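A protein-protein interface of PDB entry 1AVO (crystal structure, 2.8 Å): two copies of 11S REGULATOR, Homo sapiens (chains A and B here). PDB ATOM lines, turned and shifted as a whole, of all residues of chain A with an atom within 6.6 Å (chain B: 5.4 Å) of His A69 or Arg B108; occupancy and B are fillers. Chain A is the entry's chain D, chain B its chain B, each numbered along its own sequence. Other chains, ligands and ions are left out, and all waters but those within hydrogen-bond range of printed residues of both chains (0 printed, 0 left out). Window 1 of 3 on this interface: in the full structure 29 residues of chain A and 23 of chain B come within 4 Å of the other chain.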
ATOM      1  N   LEU A  12      15.931  27.311  39.604  1.00  0.00           N
ATOM      2  CA  LEU A  12      16.301  26.469  38.474  1.00  0.00           C
ATOM      3  C   LEU A  12      15.296  25.390  38.313  1.00  0.00           C
ATOM      4  O   LEU A  12      14.951  25.021  37.199  1.00  0.00           O
ATOM      5  CB  LEU A  12      17.668  25.847  38.652  1.00  0.00           C
ATOM      6  CG  LEU A  12      18.815  26.846  38.493  1.00  0.00           C
ATOM      7  CD1 LEU A  12      20.100  26.110  38.676  1.00  0.00           C
ATOM      8  CD2 LEU A  12      18.795  27.499  37.126  1.00  0.00           C
ATOM      9  N   GLN A  13      14.823  24.875  39.421  1.00  0.00           N
ATOM     10  CA  GLN A  13      13.844  23.809  39.356  1.00  0.00           C
ATOM     11  C   GLN A  13      12.574  24.200  38.594  1.00  0.00           C
ATOM     12  O   GLN A  13      11.944  23.357  37.935  1.00  0.00           O
ATOM     13  CB  GLN A  13      13.432  23.325  40.762  1.00  0.00           C
ATOM     14  CG  GLN A  13      14.501  22.636  41.554  1.00  0.00           C
ATOM     15  CD  GLN A  13      15.314  21.659  40.705  1.00  0.00           C
ATOM     16  OE1 GLN A  13      14.804  20.613  40.292  1.00  0.00           O
ATOM     17  NE2 GLN A  13      16.592  22.001  40.433  1.00  0.00           N
ATOM     18  N   LYS A  16      13.818  24.984  34.530  1.00  0.00           N
ATOM     19  CA  LYS A  16      14.093  23.907  33.604  1.00  0.00           C
ATOM     20  C   LYS A  16      12.926  23.372  32.819  1.00  0.00           C
ATOM     21  O   LYS A  16      12.993  23.211  31.618  1.00  0.00           O
ATOM     22  CB  LYS A  16      14.819  22.823  34.306  1.00  0.00           C
ATOM     23  CG  LYS A  16      16.161  23.277  34.703  1.00  0.00           C
ATOM     24  CD  LYS A  16      16.948  22.134  35.250  1.00  0.00           C
ATOM     25  CE  LYS A  16      16.367  21.603  36.542  1.00  0.00           C
ATOM     26  NZ  LYS A  16      17.345  20.733  37.260  1.00  0.00           N
ATOM     27  N   PRO A  17      11.785  23.223  33.469  1.00  0.00           N
ATOM     28  CA  PRO A  17      10.621  22.713  32.743  1.00  0.00           C
ATOM     29  C   PRO A  17      10.109  23.694  31.718  1.00  0.00           C
ATOM     30  O   PRO A  17       9.603  23.307  30.676  1.00  0.00           O
ATOM     31  CB  PRO A  17       9.614  22.537  33.851  1.00  0.00           C
ATOM     32  CG  PRO A  17      10.495  22.280  35.049  1.00  0.00           C
ATOM     33  CD  PRO A  17      11.516  23.311  34.900  1.00  0.00           C
ATOM     34  N   GLU A  18      10.215  24.978  32.023  1.00  0.00           N
ATOM     35  CA  GLU A  18       9.713  25.999  31.103  1.00  0.00           C
ATOM     36  C   GLU A  18      10.520  26.038  29.843  1.00  0.00           C
ATOM     37  O   GLU A  18       9.967  26.296  28.765  1.00  0.00           O
ATOM     38  CB  GLU A  18       9.664  27.361  31.759  1.00  0.00           C
ATOM     39  CG  GLU A  18       8.654  27.454  32.893  1.00  0.00           C
ATOM     40  CD  GLU A  18       7.261  27.009  32.492  1.00  0.00           C
ATOM     41  OE1 GLU A  18       6.756  27.450  31.431  1.00  0.00           O
ATOM     42  OE2 GLU A  18       6.683  26.188  33.238  1.00  0.00           O
ATOM     43  N   ILE A  19      11.811  25.720  29.986  1.00  0.00           N
ATOM     44  CA  ILE A  19      12.741  25.686  28.855  1.00  0.00           C
ATOM     45  C   ILE A  19      12.387  24.498  28.018  1.00  0.00           C
ATOM     46  O   ILE A  19      12.328  24.607  26.832  1.00  0.00           O
ATOM     47  CB  ILE A  19      14.222  25.487  29.266  1.00  0.00           C
ATOM     48  CG1 ILE A  19      14.713  26.671  30.061  1.00  0.00           C
ATOM     49  CG2 ILE A  19      15.097  25.392  28.061  1.00  0.00           C
ATOM     50  CD1 ILE A  19      16.081  26.495  30.563  1.00  0.00           C
ATOM     51  N   LYS A  20      12.226  23.341  28.638  1.00  0.00           N
ATOM     52  CA  LYS A  20      11.862  22.149  27.912  1.00  0.00           C
ATOM     53  C   LYS A  20      10.565  22.404  27.132  1.00  0.00           C
ATOM     54  O   LYS A  20      10.452  21.981  25.990  1.00  0.00           O
ATOM     55  CB  LYS A  20      11.686  20.987  28.884  1.00  0.00           C
ATOM     56  CG  LYS A  20      11.225  19.710  28.206  1.00  0.00           C
ATOM     57  CD  LYS A  20      10.571  18.704  29.180  1.00  0.00           C
ATOM     58  CE  LYS A  20       9.925  17.534  28.405  1.00  0.00           C
ATOM     59  NZ  LYS A  20       9.316  16.453  29.278  1.00  0.00           N
ATOM     60  N   ILE A  23      11.193  24.790  23.841  1.00  0.00           N
ATOM     61  CA  ILE A  23      11.929  24.077  22.822  1.00  0.00           C
ATOM     62  C   ILE A  23      11.030  23.054  22.148  1.00  0.00           C
ATOM     63  O   ILE A  23      11.191  22.803  20.979  1.00  0.00           O
ATOM     64  CB  ILE A  23      13.153  23.334  23.329  1.00  0.00           C
ATOM     65  CG1 ILE A  23      14.063  24.211  24.167  1.00  0.00           C
ATOM     66  CG2 ILE A  23      13.935  22.889  22.172  1.00  0.00           C
ATOM     67  CD1 ILE A  23      14.845  25.168  23.361  1.00  0.00           C
ATOM     68  N   GLU A  24      10.108  22.426  22.854  1.00  0.00           N
ATOM     69  CA  GLU A  24       9.235  21.462  22.180  1.00  0.00           C
ATOM     70  C   GLU A  24       8.164  22.112  21.335  1.00  0.00           C
ATOM     71  O   GLU A  24       7.874  21.674  20.246  1.00  0.00           O
ATOM     72  CB  GLU A  24       8.598  20.498  23.167  1.00  0.00           C
ATOM     73  CG  GLU A  24       9.592  19.436  23.721  1.00  0.00           C
ATOM     74  CD  GLU A  24       8.910  18.307  24.552  1.00  0.00           C
ATOM     75  OE1 GLU A  24       7.627  18.198  24.574  1.00  0.00           O
ATOM     76  OE2 GLU A  24       9.681  17.522  25.169  1.00  0.00           O
ATOM     77  N   LEU A  65      17.178  29.836  22.439  1.00  0.00           N
ATOM     78  CA  LEU A  65      16.706  28.985  23.516  1.00  0.00           C
ATOM     79  C   LEU A  65      17.425  27.681  23.752  1.00  0.00           C
ATOM     80  O   LEU A  65      17.379  27.126  24.837  1.00  0.00           O
ATOM     81  CB  LEU A  65      15.250  28.675  23.299  1.00  0.00           C
ATOM     82  CG  LEU A  65      14.390  29.905  23.220  1.00  0.00           C
ATOM     83  CD1 LEU A  65      13.053  29.406  22.904  1.00  0.00           C
ATOM     84  CD2 LEU A  65      14.404  30.688  24.510  1.00  0.00           C
ATOM     85  N   GLU A  66      18.050  27.146  22.731  1.00  0.00           N
ATOM     86  CA  GLU A  66      18.749  25.885  22.900  1.00  0.00           C
ATOM     87  C   GLU A  66      19.906  26.036  23.903  1.00  0.00           C
ATOM     88  O   GLU A  66      20.221  25.124  24.668  1.00  0.00           O
ATOM     89  CB  GLU A  66      19.269  25.425  21.556  1.00  0.00           C
ATOM     90  CG  GLU A  66      19.617  23.957  21.523  1.00  0.00           C
ATOM     91  CD  GLU A  66      19.848  23.436  20.096  1.00  0.00           C
ATOM     92  OE1 GLU A  66      20.318  24.233  19.229  1.00  0.00           O
ATOM     93  OE2 GLU A  66      19.551  22.229  19.852  1.00  0.00           O
ATOM     94  N   GLY A  67      20.511  27.217  23.921  1.00  0.00           N
ATOM     95  CA  GLY A  67      21.622  27.466  24.815  1.00  0.00           C
ATOM     96  C   GLY A  67      21.258  27.379  26.275  1.00  0.00           C
ATOM     97  O   GLY A  67      22.003  26.816  27.052  1.00  0.00           O
ATOM     98  N   PHE A  68      20.104  27.931  26.631  1.00  0.00           N
ATOM     99  CA  PHE A  68      19.632  27.951  27.997  1.00  0.00           C
ATOM    100  C   PHE A  68      19.749  26.618  28.666  1.00  0.00           C
ATOM    101  O   PHE A  68      20.172  26.524  29.810  1.00  0.00           O
ATOM    102  CB  PHE A  68      18.168  28.333  28.057  1.00  0.00           C
ATOM    103  CG  PHE A  68      17.866  29.717  27.603  1.00  0.00           C
ATOM    104  CD1 PHE A  68      18.871  30.562  27.158  1.00  0.00           C
ATOM    105  CD2 PHE A  68      16.553  30.190  27.647  1.00  0.00           C
ATOM    106  CE1 PHE A  68      18.565  31.867  26.763  1.00  0.00           C
ATOM    107  CE2 PHE A  68      16.246  31.459  27.258  1.00  0.00           C
ATOM    108  CZ  PHE A  68      17.248  32.312  26.815  1.00  0.00           C
ATOM    109  N   HIS A  69      19.341  25.577  27.983  1.00  0.00           N
ATOM    110  CA  HIS A  69      19.408  24.278  28.623  1.00  0.00           C
ATOM    111  C   HIS A  69      20.753  24.001  29.296  1.00  0.00           C
ATOM    112  O   HIS A  69      20.852  23.791  30.506  1.00  0.00           O
ATOM    113  CB  HIS A  69      19.099  23.178  27.596  1.00  0.00           C
ATOM    114  CG  HIS A  69      17.925  22.324  27.971  1.00  0.00           C
ATOM    115  ND1 HIS A  69      17.623  22.021  29.289  1.00  0.00           N
ATOM    116  CD2 HIS A  69      16.939  21.785  27.224  1.00  0.00           C
ATOM    117  CE1 HIS A  69      16.498  21.338  29.330  1.00  0.00           C
ATOM    118  NE2 HIS A  69      16.057  21.178  28.095  1.00  0.00           N
ATOM    119  N   THR A  70      21.797  24.139  28.488  1.00  0.00           N
ATOM    120  CA  THR A  70      23.170  23.875  28.889  1.00  0.00           C
ATOM    121  C   THR A  70      23.780  24.869  29.869  1.00  0.00           C
ATOM    122  O   THR A  70      24.678  24.517  30.593  1.00  0.00           O
ATOM    123  CB  THR A  70      24.074  23.773  27.642  1.00  0.00           C
ATOM    124  OG1 THR A  70      24.278  25.077  27.097  1.00  0.00           O
ATOM    125  CG2 THR A  70      23.411  22.936  26.536  1.00  0.00           C
ATOM    126  N   GLN A  71      23.308  26.110  29.887  1.00  0.00           N
ATOM    127  CA  GLN A  71      23.830  27.136  30.794  1.00  0.00           C
ATOM    128  C   GLN A  71      23.636  26.782  32.268  1.00  0.00           C
ATOM    129  O   GLN A  71      24.262  27.358  33.158  1.00  0.00           O
ATOM    130  CB  GLN A  71      23.132  28.479  30.510  1.00  0.00           C
ATOM    131  CG  GLN A  71      23.433  29.052  29.111  1.00  0.00           C
ATOM    132  CD  GLN A  71      22.717  30.374  28.808  1.00  0.00           C
ATOM    133  OE1 GLN A  71      22.310  31.104  29.727  1.00  0.00           O
ATOM    134  NE2 GLN A  71      22.570  30.689  27.510  1.00  0.00           N
ATOM    135  N   ILE A  72      22.751  25.823  32.503  1.00  0.00           N
ATOM    136  CA  ILE A  72      22.417  25.392  33.842  1.00  0.00           C
ATOM    137  C   ILE A  72      23.442  24.439  34.442  1.00  0.00           C
ATOM    138  O   ILE A  72      23.780  24.564  35.592  1.00  0.00           O
ATOM    139  CB  ILE A  72      20.990  24.793  33.858  1.00  0.00           C
ATOM    140  CG1 ILE A  72      19.967  25.917  33.576  1.00  0.00           C
ATOM    141  CG2 ILE A  72      20.738  24.069  35.190  1.00  0.00           C
ATOM    142  CD1 ILE A  72      18.602  25.452  33.175  1.00  0.00           C
ATOM    143  N   SER A  73      23.943  23.500  33.651  1.00  0.00           N
ATOM    144  CA  SER A  73      24.927  22.543  34.122  1.00  0.00           C
ATOM    145  C   SER A  73      26.196  23.279  34.324  1.00  0.00           C
ATOM    146  O   SER A  73      26.918  23.000  35.265  1.00  0.00           O
ATOM    147  CB  SER A  73      25.181  21.458  33.102  1.00  0.00           C
ATOM    148  OG  SER A  73      23.970  20.829  32.791  1.00  0.00           O
ATOM    149  N   LYS A  74      26.482  24.200  33.422  1.00  0.00           N
ATOM    150  CA  LYS A  74      27.677  25.026  33.509  1.00  0.00           C
ATOM    151  C   LYS A  74      27.717  25.745  34.851  1.00  0.00           C
ATOM    152  O   LYS A  74      28.755  25.833  35.449  1.00  0.00           O
ATOM    153  CB  LYS A  74      27.714  26.052  32.381  1.00  0.00           C
ATOM    154  CG  LYS A  74      29.021  26.859  32.304  1.00  0.00           C
ATOM    155  CD  LYS A  74      28.972  27.856  31.145  1.00  0.00           C
ATOM    156  CE  LYS A  74      30.252  28.682  30.983  1.00  0.00           C
ATOM    157  NZ  LYS A  74      30.327  29.427  29.655  1.00  0.00           N
ATOM    158  N   MET A 113      16.350  34.610  31.369  1.00  0.00           N
ATOM    159  CA  MET A 113      15.874  33.477  30.608  1.00  0.00           C
ATOM    160  C   MET A 113      14.380  33.406  30.675  1.00  0.00           C
ATOM    161  O   MET A 113      13.747  33.057  29.696  1.00  0.00           O
ATOM    162  CB  MET A 113      16.457  32.162  31.111  1.00  0.00           C
ATOM    163  CG  MET A 113      17.982  32.121  31.039  1.00  0.00           C
ATOM    164  SD  MET A 113      18.713  30.490  31.180  1.00  0.00           S
ATOM    165  CE  MET A 113      19.357  30.525  32.780  1.00  0.00           C
ATOM    166  N   ASP B 103      21.977  14.038  34.022  1.00  0.00           N
ATOM    167  CA  ASP B 103      21.017  12.994  33.727  1.00  0.00           C
ATOM    168  C   ASP B 103      19.711  13.602  33.283  1.00  0.00           C
ATOM    169  O   ASP B 103      19.124  13.186  32.302  1.00  0.00           O
ATOM    170  CB  ASP B 103      20.789  12.104  34.945  1.00  0.00           C
ATOM    171  CG  ASP B 103      21.985  11.240  35.275  1.00  0.00           C
ATOM    172  OD1 ASP B 103      22.896  11.152  34.445  1.00  0.00           O
ATOM    173  OD2 ASP B 103      22.019  10.624  36.357  1.00  0.00           O
ATOM    174  N   GLU B 104      19.266  14.633  33.981  1.00  0.00           N
ATOM    175  CA  GLU B 104      18.009  15.260  33.615  1.00  0.00           C
ATOM    176  C   GLU B 104      18.109  15.807  32.242  1.00  0.00           C
ATOM    177  O   GLU B 104      17.213  15.634  31.443  1.00  0.00           O
ATOM    178  CB  GLU B 104      17.662  16.384  34.556  1.00  0.00           C
ATOM    179  CG  GLU B 104      16.869  15.912  35.733  1.00  0.00           C
ATOM    180  CD  GLU B 104      16.387  17.047  36.598  1.00  0.00           C
ATOM    181  OE1 GLU B 104      16.231  18.185  36.101  1.00  0.00           O
ATOM    182  OE2 GLU B 104      16.146  16.802  37.802  1.00  0.00           O
ATOM    183  N   ALA B 105      19.236  16.433  31.944  1.00  0.00           N
ATOM    184  CA  ALA B 105      19.416  16.999  30.624  1.00  0.00           C
ATOM    185  C   ALA B 105      19.501  15.927  29.599  1.00  0.00           C
ATOM    186  O   ALA B 105      18.885  16.046  28.582  1.00  0.00           O
ATOM    187  CB  ALA B 105      20.612  17.826  30.558  1.00  0.00           C
ATOM    188  N   GLU B 106      20.215  14.840  29.861  1.00  0.00           N
ATOM    189  CA  GLU B 106      20.316  13.810  28.832  1.00  0.00           C
ATOM    190  C   GLU B 106      18.924  13.269  28.585  1.00  0.00           C
ATOM    191  O   GLU B 106      18.547  12.970  27.466  1.00  0.00           O
ATOM    192  CB  GLU B 106      21.301  12.718  29.201  1.00  0.00           C
ATOM    193  CG  GLU B 106      21.598  11.760  28.057  1.00  0.00           C
ATOM    194  CD  GLU B 106      22.306  12.404  26.845  1.00  0.00           C
ATOM    195  OE1 GLU B 106      22.713  13.585  26.942  1.00  0.00           O
ATOM    196  OE2 GLU B 106      22.461  11.744  25.782  1.00  0.00           O
ATOM    197  N   TYR B 107      18.109  13.271  29.620  1.00  0.00           N
ATOM    198  CA  TYR B 107      16.779  12.764  29.436  1.00  0.00           C
ATOM    199  C   TYR B 107      15.986  13.734  28.571  1.00  0.00           C
ATOM    200  O   TYR B 107      15.294  13.328  27.657  1.00  0.00           O
ATOM    201  CB  TYR B 107      16.112  12.520  30.773  1.00  0.00           C
ATOM    202  CG  TYR B 107      14.674  12.113  30.609  1.00  0.00           C
ATOM    203  CD1 TYR B 107      14.322  10.767  30.426  1.00  0.00           C
ATOM    204  CD2 TYR B 107      13.652  13.081  30.566  1.00  0.00           C
ATOM    205  CE1 TYR B 107      12.995  10.395  30.195  1.00  0.00           C
ATOM    206  CE2 TYR B 107      12.320  12.715  30.335  1.00  0.00           C
ATOM    207  CZ  TYR B 107      12.014  11.373  30.149  1.00  0.00           C
ATOM    208  OH  TYR B 107      10.725  11.008  29.881  1.00  0.00           O
ATOM    209  N   ARG B 108      16.132  15.028  28.826  1.00  0.00           N
ATOM    210  CA  ARG B 108      15.411  16.017  28.045  1.00  0.00           C
ATOM    211  C   ARG B 108      15.816  16.039  26.603  1.00  0.00           C
ATOM    212  O   ARG B 108      15.006  16.363  25.754  1.00  0.00           O
ATOM    213  CB  ARG B 108      15.550  17.386  28.647  1.00  0.00           C
ATOM    214  CG  ARG B 108      14.829  17.466  29.971  1.00  0.00           C
ATOM    215  CD  ARG B 108      14.639  18.932  30.444  1.00  0.00           C
ATOM    216  NE  ARG B 108      14.979  19.196  31.862  1.00  0.00           N
ATOM    217  CZ  ARG B 108      14.086  19.272  32.865  1.00  0.00           C
ATOM    218  NH1 ARG B 108      12.771  19.108  32.662  1.00  0.00           N
ATOM    219  NH2 ARG B 108      14.506  19.500  34.103  1.00  0.00           N
ATOM    220  N   ASP B 109      17.054  15.634  26.334  1.00  0.00           N
ATOM    221  CA  ASP B 109      17.622  15.589  24.975  1.00  0.00           C
ATOM    222  C   ASP B 109      17.140  14.407  24.190  1.00  0.00           C
ATOM    223  O   ASP B 109      16.825  14.537  23.011  1.00  0.00           O
ATOM    224  CB  ASP B 109      19.122  15.481  25.006  1.00  0.00           C
ATOM    225  CG  ASP B 109      19.802  16.784  25.411  1.00  0.00           C
ATOM    226  OD1 ASP B 109      19.141  17.850  25.285  1.00  0.00           O
ATOM    227  OD2 ASP B 109      21.003  16.744  25.841  1.00  0.00           O
ATOM    228  N   ILE B 110      17.159  13.233  24.810  1.00  0.00           N
ATOM    229  CA  ILE B 110      16.675  12.049  24.145  1.00  0.00           C
ATOM    230  C   ILE B 110      15.274  12.306  23.591  1.00  0.00           C
ATOM    231  O   ILE B 110      14.973  11.977  22.453  1.00  0.00           O
ATOM    232  CB  ILE B 110      16.581  10.900  25.089  1.00  0.00           C
ATOM    233  CG1 ILE B 110      17.949  10.584  25.671  1.00  0.00           C
ATOM    234  CG2 ILE B 110      16.004   9.716  24.375  1.00  0.00           C
ATOM    235  CD1 ILE B 110      17.904   9.432  26.666  1.00  0.00           C
ATOM    236  N   ARG B 111      14.417  12.925  24.396  1.00  0.00           N
ATOM    237  CA  ARG B 111      13.068  13.207  23.946  1.00  0.00           C
ATOM    238  C   ARG B 111      13.151  14.126  22.743  1.00  0.00           C
ATOM    239  O   ARG B 111      12.537  13.875  21.734  1.00  0.00           O
ATOM    240  CB  ARG B 111      12.252  13.819  25.065  1.00  0.00           C
ATOM    241  CG  ARG B 111      10.859  14.078  24.622  1.00  0.00           C
ATOM    242  CD  ARG B 111       9.916  14.401  25.750  1.00  0.00           C
ATOM    243  NE  ARG B 111       8.648  13.723  25.511  1.00  0.00           N
ATOM    244  CZ  ARG B 111       7.705  14.154  24.699  1.00  0.00           C
ATOM    245  NH1 ARG B 111       7.876  15.296  24.064  1.00  0.00           N
ATOM    246  NH2 ARG B 111       6.648  13.385  24.427  1.00  0.00           N
ATOM    247  N   LEU B 112      13.971  15.157  22.835  1.00  0.00           N
ATOM    248  CA  LEU B 112      14.151  16.066  21.734  1.00  0.00           C
ATOM    249  C   LEU B 112      14.771  15.423  20.524  1.00  0.00           C
ATOM    250  O   LEU B 112      14.439  15.816  19.417  1.00  0.00           O
ATOM    251  CB  LEU B 112      15.033  17.191  22.141  1.00  0.00           C
ATOM    252  CG  LEU B 112      14.299  18.380  22.694  1.00  0.00           C
ATOM    253  CD1 LEU B 112      15.322  19.353  23.164  1.00  0.00           C
ATOM    254  CD2 LEU B 112      13.525  19.015  21.590  1.00  0.00           C
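Hydrophobic or aromatic side chains of chain A that line the printed part of chain B: Ile A23 and His A69. Of the 10 printed residues of chain B, 4 touch a printed residue of chain A.
The side-chain carboxylate of Glu B104 is in salt-bridge range of the guanidinium group of Arg B108. The side-chain amide nitrogen of Gln A13 sits close to the side-chain amino group of Lys A16.
The side-chain amino group (NZ) of Lys A16 is in salt-bridge range of the side-chain carboxylate (OE1) of Glu B104, 3.0 Å away. The side-chain carboxylate (OE1) of Glu A24 lies within salt-bridge range of the guanidinium group (NH1) of Arg B111.
Among the printed residues, pairs that only touch across the chains: Lys A16 with Arg B108 (3.3 Å), Lys A20 with Arg B108 (3.9 Å), Ile A23 with Leu B112 (3.9 Å) and His A69 with Arg B108 (3.2 Å).
Of the printed residues of chain A, Leu B112 touches Ile A23. Of the printed residues of chain A, Glu B104 touches Lys A16. Phe A68 touches none of the printed residues of chain B. The nearest residue of chain A that does not touch Arg B108 is Pro A17 (4.2 Å). The nearest printed residue of chain A that does not touch Arg B111 is Lys A20 (4.1 Å).
No position is printed for both chains. Of the 6 pairs that touch across the chains among the printed residues, none has its exchanged pair printed and touching as well.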
